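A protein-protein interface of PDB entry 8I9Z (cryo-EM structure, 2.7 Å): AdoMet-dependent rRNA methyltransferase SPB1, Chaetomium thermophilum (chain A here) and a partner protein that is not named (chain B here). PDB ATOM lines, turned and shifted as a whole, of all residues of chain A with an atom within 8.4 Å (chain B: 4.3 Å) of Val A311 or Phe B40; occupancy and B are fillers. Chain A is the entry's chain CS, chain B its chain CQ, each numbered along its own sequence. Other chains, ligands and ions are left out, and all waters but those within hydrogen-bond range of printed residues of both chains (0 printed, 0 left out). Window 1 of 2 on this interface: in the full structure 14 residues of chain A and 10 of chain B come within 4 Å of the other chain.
Of the 16 printed residues of chain A, 6 touch a printed residue of chain B.
Printed residues of chain A that touch a printed residue of chain B: Pro A235, Glu A236, Lys A310, Val A311, Leu A312 and Gly A313.
Among the printed residues, 6 pairs touch across the chains.
Of the printed residues of chain B, Pro A235 touches Lys B43 (3.3 Å).
Printed residues of chain B within 4 Å of Glu A236: Met B42.
Cys A305 touches none of the printed residues of chain B.
Of the printed residues of chain B, Lys A310 touches Lys B43 (3.4 Å).
Val A311 touches just one residue of chain B: Phe B40 (3.7 Å).
Of the printed residues of chain B, Leu A312 touches Lys B43 (3.3 Å).
Phe B40 touches just one residue of chain A: Val A311 (3.7 Å).
Printed residues of chain A within 4 Å of Lys B43: Pro A235 (3.3 Å), Lys A310 (3.4 Å), Leu A312 (3.3 Å) and Gly A313 (3.7 Å).
The nearest printed residue of chain A that does not touch Met B42 is Gly A313 (5.9 Å).
The backbone carbonyl oxygen (O) of Met B42 lies close to the side-chain carboxylate (OE2) of Glu A236 (3.1 Å).
The side-chain amino group (NZ) of Lys A310 lies close to the side-chain amide nitrogen (ND2) of Asn A275 (3.4 Å).
Among the printed residues, merely in contact across the chains: Pro A235 with Lys B43 (3.3 Å), Leu A312 with Lys B43 (3.3 Å), Lys A310 with Lys B43 (3.4 Å), Gly A313 with Lys B43 (3.7 Å) and Val A311 with Phe B40 (3.7 Å).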
ATOM      1  N   PRO A 235      25.806   2.975  -6.791  1.00  0.00           N
ATOM      2  CA  PRO A 235      26.748   3.637  -7.708  1.00  0.00           C
ATOM      3  C   PRO A 235      27.149   5.057  -7.327  1.00  0.00           C
ATOM      4  O   PRO A 235      27.917   5.669  -8.075  1.00  0.00           O
ATOM      5  CB  PRO A 235      25.961   3.643  -9.023  1.00  0.00           C
ATOM      6  CG  PRO A 235      24.509   3.552  -8.630  1.00  0.00           C
ATOM      7  CD  PRO A 235      24.412   3.251  -7.163  1.00  0.00           C
ATOM      8  N   GLU A 236      26.678   5.582  -6.196  1.00  0.00           N
ATOM      9  CA  GLU A 236      27.053   6.899  -5.677  1.00  0.00           C
ATOM     10  C   GLU A 236      28.336   6.866  -4.880  1.00  0.00           C
ATOM     11  O   GLU A 236      28.689   7.829  -4.191  1.00  0.00           O
ATOM     12  CB  GLU A 236      25.924   7.452  -4.807  1.00  0.00           C
ATOM     13  CG  GLU A 236      24.567   7.478  -5.487  1.00  0.00           C
ATOM     14  CD  GLU A 236      23.488   8.085  -4.612  1.00  0.00           C
ATOM     15  OE1 GLU A 236      23.764   8.351  -3.423  1.00  0.00           O
ATOM     16  OE2 GLU A 236      22.364   8.298  -5.112  1.00  0.00           O
ATOM     17  N   TYR A 274      28.427  -2.182 -19.228  1.00  0.00           N
ATOM     18  CA  TYR A 274      28.106  -1.674 -20.555  1.00  0.00           C
ATOM     19  C   TYR A 274      27.493  -0.281 -20.472  1.00  0.00           C
ATOM     20  O   TYR A 274      26.901   0.105 -19.462  1.00  0.00           O
ATOM     21  CB  TYR A 274      27.172  -2.628 -21.321  1.00  0.00           C
ATOM     22  CG  TYR A 274      27.785  -3.962 -21.776  1.00  0.00           C
ATOM     23  CD1 TYR A 274      27.428  -4.529 -22.989  1.00  0.00           C
ATOM     24  CD2 TYR A 274      28.695  -4.662 -20.985  1.00  0.00           C
ATOM     25  CE1 TYR A 274      27.979  -5.731 -23.403  1.00  0.00           C
ATOM     26  CE2 TYR A 274      29.242  -5.861 -21.389  1.00  0.00           C
ATOM     27  CZ  TYR A 274      28.878  -6.393 -22.598  1.00  0.00           C
ATOM     28  OH  TYR A 274      29.420  -7.590 -23.006  1.00  0.00           O
ATOM     29  N   ASN A 275      27.647   0.474 -21.558  1.00  0.00           N
ATOM     30  CA  ASN A 275      27.298   1.888 -21.590  1.00  0.00           C
ATOM     31  C   ASN A 275      25.863   2.146 -22.024  1.00  0.00           C
ATOM     32  O   ASN A 275      25.224   3.066 -21.508  1.00  0.00           O
ATOM     33  CB  ASN A 275      28.243   2.637 -22.530  1.00  0.00           C
ATOM     34  CG  ASN A 275      29.381   3.306 -21.802  1.00  0.00           C
ATOM     35  OD1 ASN A 275      30.538   2.920 -21.951  1.00  0.00           O
ATOM     36  ND2 ASN A 275      29.061   4.317 -21.004  1.00  0.00           N
ATOM     37  N   ALA A 304      14.815   6.580 -21.391  1.00  0.00           N
ATOM     38  CA  ALA A 304      15.815   7.575 -21.022  1.00  0.00           C
ATOM     39  C   ALA A 304      16.960   6.953 -20.232  1.00  0.00           C
ATOM     40  O   ALA A 304      18.119   7.349 -20.396  1.00  0.00           O
ATOM     41  CB  ALA A 304      15.165   8.704 -20.226  1.00  0.00           C
ATOM     42  N   CYS A 305      16.658   5.985 -19.364  1.00  0.00           N
ATOM     43  CA  CYS A 305      17.710   5.322 -18.600  1.00  0.00           C
ATOM     44  C   CYS A 305      18.547   4.408 -19.484  1.00  0.00           C
ATOM     45  O   CYS A 305      19.737   4.200 -19.220  1.00  0.00           O
ATOM     46  CB  CYS A 305      17.107   4.532 -17.439  1.00  0.00           C
ATOM     47  SG  CYS A 305      16.401   5.539 -16.120  1.00  0.00           S
ATOM     48  N   ASP A 307      19.451   4.965 -22.523  1.00  0.00           N
ATOM     49  CA  ASP A 307      20.343   5.711 -23.402  1.00  0.00           C
ATOM     50  C   ASP A 307      21.683   5.986 -22.729  1.00  0.00           C
ATOM     51  O   ASP A 307      22.729   5.982 -23.388  1.00  0.00           O
ATOM     52  CB  ASP A 307      19.681   7.017 -23.829  1.00  0.00           C
ATOM     53  CG  ASP A 307      18.883   6.874 -25.110  1.00  0.00           C
ATOM     54  OD1 ASP A 307      18.411   5.754 -25.398  1.00  0.00           O
ATOM     55  OD2 ASP A 307      18.725   7.883 -25.830  1.00  0.00           O
ATOM     56  N   ASP A 308      21.671   6.233 -21.418  1.00  0.00           N
ATOM     57  CA  ASP A 308      22.861   6.624 -20.659  1.00  0.00           C
ATOM     58  C   ASP A 308      22.880   5.820 -19.363  1.00  0.00           C
ATOM     59  O   ASP A 308      22.313   6.234 -18.351  1.00  0.00           O
ATOM     60  CB  ASP A 308      22.859   8.130 -20.394  1.00  0.00           C
ATOM     61  CG  ASP A 308      24.256   8.715 -20.337  1.00  0.00           C
ATOM     62  OD1 ASP A 308      25.232   7.940 -20.394  1.00  0.00           O
ATOM     63  OD2 ASP A 308      24.375   9.955 -20.233  1.00  0.00           O
ATOM     64  N   LEU A 309      23.538   4.662 -19.397  1.00  0.00           N
ATOM     65  CA  LEU A 309      23.571   3.804 -18.219  1.00  0.00           C
ATOM     66  C   LEU A 309      24.554   4.303 -17.172  1.00  0.00           C
ATOM     67  O   LEU A 309      24.384   4.016 -15.981  1.00  0.00           O
ATOM     68  CB  LEU A 309      23.922   2.372 -18.613  1.00  0.00           C
ATOM     69  CG  LEU A 309      22.782   1.399 -18.897  1.00  0.00           C
ATOM     70  CD1 LEU A 309      22.083   1.724 -20.200  1.00  0.00           C
ATOM     71  CD2 LEU A 309      23.339   0.001 -18.938  1.00  0.00           C
ATOM     72  N   LYS A 310      25.581   5.037 -17.584  1.00  0.00           N
ATOM     73  CA  LYS A 310      26.681   5.380 -16.695  1.00  0.00           C
ATOM     74  C   LYS A 310      26.333   6.497 -15.715  1.00  0.00           C
ATOM     75  O   LYS A 310      27.083   6.716 -14.758  1.00  0.00           O
ATOM     76  CB  LYS A 310      27.908   5.756 -17.532  1.00  0.00           C
ATOM     77  CG  LYS A 310      29.240   5.570 -16.832  1.00  0.00           C
ATOM     78  CD  LYS A 310      29.419   4.133 -16.375  1.00  0.00           C
ATOM     79  CE  LYS A 310      29.559   3.189 -17.551  1.00  0.00           C
ATOM     80  NZ  LYS A 310      30.830   3.408 -18.289  1.00  0.00           N
ATOM     81  N   VAL A 311      25.210   7.184 -15.903  1.00  0.00           N
ATOM     82  CA  VAL A 311      24.826   8.295 -15.048  1.00  0.00           C
ATOM     83  C   VAL A 311      23.675   7.917 -14.115  1.00  0.00           C
ATOM     84  O   VAL A 311      23.076   8.789 -13.494  1.00  0.00           O
ATOM     85  CB  VAL A 311      24.471   9.537 -15.878  1.00  0.00           C
ATOM     86  CG1 VAL A 311      25.674  10.008 -16.667  1.00  0.00           C
ATOM     87  CG2 VAL A 311      23.314   9.233 -16.802  1.00  0.00           C
ATOM     88  N   LEU A 312      23.355   6.633 -14.002  1.00  0.00           N
ATOM     89  CA  LEU A 312      22.171   6.212 -13.268  1.00  0.00           C
ATOM     90  C   LEU A 312      22.481   5.989 -11.791  1.00  0.00           C
ATOM     91  O   LEU A 312      23.626   5.781 -11.389  1.00  0.00           O
ATOM     92  CB  LEU A 312      21.584   4.944 -13.883  1.00  0.00           C
ATOM     93  CG  LEU A 312      21.096   5.075 -15.324  1.00  0.00           C
ATOM     94  CD1 LEU A 312      20.487   3.768 -15.799  1.00  0.00           C
ATOM     95  CD2 LEU A 312      20.098   6.206 -15.448  1.00  0.00           C
ATOM     96  N   GLY A 313      21.428   6.026 -10.979  1.00  0.00           N
ATOM     97  CA  GLY A 313      21.549   5.816  -9.551  1.00  0.00           C
ATOM     98  C   GLY A 313      20.924   4.519  -9.082  1.00  0.00           C
ATOM     99  O   GLY A 313      20.719   3.601  -9.879  1.00  0.00           O
ATOM    100  N   LYS A 314      20.624   4.436  -7.783  1.00  0.00           N
ATOM    101  CA  LYS A 314      20.057   3.216  -7.215  1.00  0.00           C
ATOM    102  C   LYS A 314      18.662   2.945  -7.759  1.00  0.00           C
ATOM    103  O   LYS A 314      18.337   1.813  -8.133  1.00  0.00           O
ATOM    104  CB  LYS A 314      20.012   3.325  -5.692  1.00  0.00           C
ATOM    105  CG  LYS A 314      21.253   2.841  -4.992  1.00  0.00           C
ATOM    106  CD  LYS A 314      21.616   3.747  -3.827  1.00  0.00           C
ATOM    107  CE  LYS A 314      22.231   2.957  -2.685  1.00  0.00           C
ATOM    108  NZ  LYS A 314      21.192   2.428  -1.757  1.00  0.00           N
ATOM    109  N   ASP A 316      17.210   4.063 -10.474  1.00  0.00           N
ATOM    110  CA  ASP A 316      17.146   3.846 -11.912  1.00  0.00           C
ATOM    111  C   ASP A 316      17.602   2.441 -12.279  1.00  0.00           C
ATOM    112  O   ASP A 316      17.034   1.815 -13.181  1.00  0.00           O
ATOM    113  CB  ASP A 316      17.982   4.897 -12.633  1.00  0.00           C
ATOM    114  CG  ASP A 316      17.444   6.296 -12.435  1.00  0.00           C
ATOM    115  OD1 ASP A 316      17.777   7.188 -13.243  1.00  0.00           O
ATOM    116  OD2 ASP A 316      16.685   6.506 -11.467  1.00  0.00           O
ATOM    117  N   PHE A 317      18.633   1.934 -11.604  1.00  0.00           N
ATOM    118  CA  PHE A 317      19.075   0.568 -11.854  1.00  0.00           C
ATOM    119  C   PHE A 317      18.056  -0.441 -11.348  1.00  0.00           C
ATOM    120  O   PHE A 317      17.854  -1.494 -11.965  1.00  0.00           O
ATOM    121  CB  PHE A 317      20.434   0.324 -11.204  1.00  0.00           C
ATOM    122  CG  PHE A 317      21.592   0.797 -12.029  1.00  0.00           C
ATOM    123  CD1 PHE A 317      21.709   0.425 -13.357  1.00  0.00           C
ATOM    124  CD2 PHE A 317      22.567   1.605 -11.480  1.00  0.00           C
ATOM    125  CE1 PHE A 317      22.772   0.859 -14.118  1.00  0.00           C
ATOM    126  CE2 PHE A 317      23.631   2.041 -12.235  1.00  0.00           C
ATOM    127  CZ  PHE A 317      23.733   1.666 -13.556  1.00  0.00           C
ATOM    128  N   PHE B   7      23.633  20.643 -18.882  1.00  0.00           N
ATOM    129  CA  PHE B   7      23.195  19.265 -19.079  1.00  0.00           C
ATOM    130  C   PHE B   7      22.124  18.874 -18.071  1.00  0.00           C
ATOM    131  O   PHE B   7      21.182  18.149 -18.407  1.00  0.00           O
ATOM    132  CB  PHE B   7      24.389  18.317 -18.985  1.00  0.00           C
ATOM    133  CG  PHE B   7      24.031  16.871 -19.150  1.00  0.00           C
ATOM    134  CD1 PHE B   7      23.757  16.354 -20.399  1.00  0.00           C
ATOM    135  CD2 PHE B   7      23.973  16.028 -18.056  1.00  0.00           C
ATOM    136  CE1 PHE B   7      23.427  15.027 -20.556  1.00  0.00           C
ATOM    137  CE2 PHE B   7      23.644  14.699 -18.207  1.00  0.00           C
ATOM    138  CZ  PHE B   7      23.371  14.199 -19.458  1.00  0.00           C
ATOM    139  N   PHE B   8      22.251  19.341 -16.833  1.00  0.00           N
ATOM    140  CA  PHE B   8      21.351  18.933 -15.766  1.00  0.00           C
ATOM    141  C   PHE B   8      20.016  19.666 -15.807  1.00  0.00           C
ATOM    142  O   PHE B   8      18.959  19.033 -15.746  1.00  0.00           O
ATOM    143  CB  PHE B   8      22.019  19.147 -14.407  1.00  0.00           C
ATOM    144  CG  PHE B   8      21.498  18.248 -13.331  1.00  0.00           C
ATOM    145  CD1 PHE B   8      20.404  18.620 -12.572  1.00  0.00           C
ATOM    146  CD2 PHE B   8      22.103  17.035 -13.073  1.00  0.00           C
ATOM    147  CE1 PHE B   8      19.921  17.798 -11.582  1.00  0.00           C
ATOM    148  CE2 PHE B   8      21.623  16.209 -12.081  1.00  0.00           C
ATOM    149  CZ  PHE B   8      20.529  16.592 -11.336  1.00  0.00           C
ATOM    150  N   PHE B  21      32.761  18.374 -17.247  1.00  0.00           N
ATOM    151  CA  PHE B  21      33.305  17.059 -16.936  1.00  0.00           C
ATOM    152  C   PHE B  21      33.425  16.251 -18.220  1.00  0.00           C
ATOM    153  O   PHE B  21      32.462  16.151 -18.985  1.00  0.00           O
ATOM    154  CB  PHE B  21      32.420  16.346 -15.915  1.00  0.00           C
ATOM    155  CG  PHE B  21      32.685  14.878 -15.787  1.00  0.00           C
ATOM    156  CD1 PHE B  21      33.916  14.414 -15.370  1.00  0.00           C
ATOM    157  CD2 PHE B  21      31.684  13.963 -16.047  1.00  0.00           C
ATOM    158  CE1 PHE B  21      34.151  13.067 -15.238  1.00  0.00           C
ATOM    159  CE2 PHE B  21      31.915  12.614 -15.915  1.00  0.00           C
ATOM    160  CZ  PHE B  21      33.150  12.166 -15.509  1.00  0.00           C
ATOM    161  N   PHE B  29      30.275  16.973 -20.432  1.00  0.00           N
ATOM    162  CA  PHE B  29      29.087  17.469 -19.751  1.00  0.00           C
ATOM    163  C   PHE B  29      29.354  18.871 -19.231  1.00  0.00           C
ATOM    164  O   PHE B  29      30.220  19.058 -18.372  1.00  0.00           O
ATOM    165  CB  PHE B  29      28.690  16.553 -18.598  1.00  0.00           C
ATOM    166  CG  PHE B  29      28.382  15.157 -19.015  1.00  0.00           C
ATOM    167  CD1 PHE B  29      27.113  14.816 -19.432  1.00  0.00           C
ATOM    168  CD2 PHE B  29      29.355  14.178 -18.976  1.00  0.00           C
ATOM    169  CE1 PHE B  29      26.824  13.534 -19.812  1.00  0.00           C
ATOM    170  CE2 PHE B  29      29.066  12.891 -19.353  1.00  0.00           C
ATOM    171  CZ  PHE B  29      27.799  12.575 -19.772  1.00  0.00           C
ATOM    172  N   PHE B  31      28.169  22.147 -17.149  1.00  0.00           N
ATOM    173  CA  PHE B  31      27.312  22.550 -16.046  1.00  0.00           C
ATOM    174  C   PHE B  31      27.365  24.060 -15.864  1.00  0.00           C
ATOM    175  O   PHE B  31      28.377  24.703 -16.153  1.00  0.00           O
ATOM    176  CB  PHE B  31      27.720  21.859 -14.745  1.00  0.00           C
ATOM    177  CG  PHE B  31      27.623  20.370 -14.803  1.00  0.00           C
ATOM    178  CD1 PHE B  31      26.396  19.751 -14.920  1.00  0.00           C
ATOM    179  CD2 PHE B  31      28.760  19.589 -14.743  1.00  0.00           C
ATOM    180  CE1 PHE B  31      26.307  18.383 -14.977  1.00  0.00           C
ATOM    181  CE2 PHE B  31      28.676  18.222 -14.799  1.00  0.00           C
ATOM    182  CZ  PHE B  31      27.449  17.619 -14.917  1.00  0.00           C
ATOM    183  N   CYS B  36      24.346  22.098  -9.847  1.00  0.00           N
ATOM    184  CA  CYS B  36      24.057  21.141 -10.905  1.00  0.00           C
ATOM    185  C   CYS B  36      25.127  20.061 -10.975  1.00  0.00           C
ATOM    186  O   CYS B  36      24.825  18.890 -11.231  1.00  0.00           O
ATOM    187  CB  CYS B  36      23.946  21.880 -12.231  1.00  0.00           C
ATOM    188  SG  CYS B  36      22.352  22.628 -12.491  1.00  0.00           S
ATOM    189  N   HIS B  37      26.383  20.441 -10.742  1.00  0.00           N
ATOM    190  CA  HIS B  37      27.494  19.501 -10.831  1.00  0.00           C
ATOM    191  C   HIS B  37      27.491  18.521  -9.669  1.00  0.00           C
ATOM    192  O   HIS B  37      27.767  17.331  -9.853  1.00  0.00           O
ATOM    193  CB  HIS B  37      28.806  20.276 -10.866  1.00  0.00           C
ATOM    194  CG  HIS B  37      30.021  19.412 -10.968  1.00  0.00           C
ATOM    195  ND1 HIS B  37      31.130  19.597 -10.174  1.00  0.00           N
ATOM    196  CD2 HIS B  37      30.316  18.381 -11.791  1.00  0.00           C
ATOM    197  CE1 HIS B  37      32.050  18.705 -10.492  1.00  0.00           C
ATOM    198  NE2 HIS B  37      31.580  17.955 -11.470  1.00  0.00           N
ATOM    199  N   LYS B  38      27.207  19.006  -8.461  1.00  0.00           N
ATOM    200  CA  LYS B  38      27.218  18.134  -7.294  1.00  0.00           C
ATOM    201  C   LYS B  38      26.079  17.124  -7.343  1.00  0.00           C
ATOM    202  O   LYS B  38      26.259  15.967  -6.951  1.00  0.00           O
ATOM    203  CB  LYS B  38      27.158  18.964  -6.014  1.00  0.00           C
ATOM    204  CG  LYS B  38      28.416  19.760  -5.749  1.00  0.00           C
ATOM    205  CD  LYS B  38      28.307  20.560  -4.477  1.00  0.00           C
ATOM    206  CE  LYS B  38      29.656  21.108  -4.062  1.00  0.00           C
ATOM    207  NZ  LYS B  38      29.550  22.496  -3.545  1.00  0.00           N
ATOM    208  N   ASN B  39      24.907  17.537  -7.826  1.00  0.00           N
ATOM    209  CA  ASN B  39      23.788  16.618  -7.982  1.00  0.00           C
ATOM    210  C   ASN B  39      24.048  15.571  -9.057  1.00  0.00           C
ATOM    211  O   ASN B  39      23.502  14.468  -8.976  1.00  0.00           O
ATOM    212  CB  ASN B  39      22.519  17.396  -8.316  1.00  0.00           C
ATOM    213  CG  ASN B  39      21.897  18.038  -7.105  1.00  0.00           C
ATOM    214  OD1 ASN B  39      21.825  17.433  -6.036  1.00  0.00           O
ATOM    215  ND2 ASN B  39      21.440  19.268  -7.259  1.00  0.00           N
ATOM    216  N   PHE B  40      24.866  15.898 -10.053  1.00  0.00           N
ATOM    217  CA  PHE B  40      25.259  14.931 -11.069  1.00  0.00           C
ATOM    218  C   PHE B  40      26.215  13.887 -10.506  1.00  0.00           C
ATOM    219  O   PHE B  40      26.111  12.704 -10.843  1.00  0.00           O
ATOM    220  CB  PHE B  40      25.897  15.667 -12.245  1.00  0.00           C
ATOM    221  CG  PHE B  40      26.346  14.776 -13.365  1.00  0.00           C
ATOM    222  CD1 PHE B  40      27.669  14.374 -13.464  1.00  0.00           C
ATOM    223  CD2 PHE B  40      25.460  14.385 -14.346  1.00  0.00           C
ATOM    224  CE1 PHE B  40      28.080  13.570 -14.497  1.00  0.00           C
ATOM    225  CE2 PHE B  40      25.871  13.587 -15.385  1.00  0.00           C
ATOM    226  CZ  PHE B  40      27.181  13.177 -15.458  1.00  0.00           C
ATOM    227  N   LYS B  41      27.158  14.309  -9.660  1.00  0.00           N
ATOM    228  CA  LYS B  41      28.166  13.386  -9.146  1.00  0.00           C
ATOM    229  C   LYS B  41      27.569  12.380  -8.179  1.00  0.00           C
ATOM    230  O   LYS B  41      28.073  11.257  -8.069  1.00  0.00           O
ATOM    231  CB  LYS B  41      29.295  14.155  -8.464  1.00  0.00           C
ATOM    232  CG  LYS B  41      30.149  14.986  -9.394  1.00  0.00           C
ATOM    233  CD  LYS B  41      31.054  15.911  -8.599  1.00  0.00           C
ATOM    234  CE  LYS B  41      32.395  15.261  -8.306  1.00  0.00           C
ATOM    235  NZ  LYS B  41      33.201  15.070  -9.543  1.00  0.00           N
ATOM    236  N   MET B  42      26.510  12.756  -7.467  1.00  0.00           N
ATOM    237  CA  MET B  42      25.807  11.800  -6.624  1.00  0.00           C
ATOM    238  C   MET B  42      24.698  11.083  -7.374  1.00  0.00           C
ATOM    239  O   MET B  42      23.892  10.393  -6.741  1.00  0.00           O
ATOM    240  CB  MET B  42      25.250  12.490  -5.377  1.00  0.00           C
ATOM    241  CG  MET B  42      24.390  13.705  -5.632  1.00  0.00           C
ATOM    242  SD  MET B  42      24.355  14.846  -4.229  1.00  0.00           S
ATOM    243  CE  MET B  42      24.577  13.735  -2.842  1.00  0.00           C
ATOM    244  N   LYS B  43      24.639  11.262  -8.695  1.00  0.00           N
ATOM    245  CA  LYS B  43      23.858  10.431  -9.612  1.00  0.00           C
ATOM    246  C   LYS B  43      22.368  10.499  -9.307  1.00  0.00           C
ATOM    247  O   LYS B  43      21.694   9.483  -9.130  1.00  0.00           O
ATOM    248  CB  LYS B  43      24.362   8.989  -9.610  1.00  0.00           C
ATOM    249  CG  LYS B  43      25.823   8.890  -9.969  1.00  0.00           C
ATOM    250  CD  LYS B  43      26.242   7.470 -10.234  1.00  0.00           C
ATOM    251  CE  LYS B  43      27.128   7.391 -11.463  1.00  0.00           C
ATOM    252  NZ  LYS B  43      28.566   7.472 -11.103  1.00  0.00           N
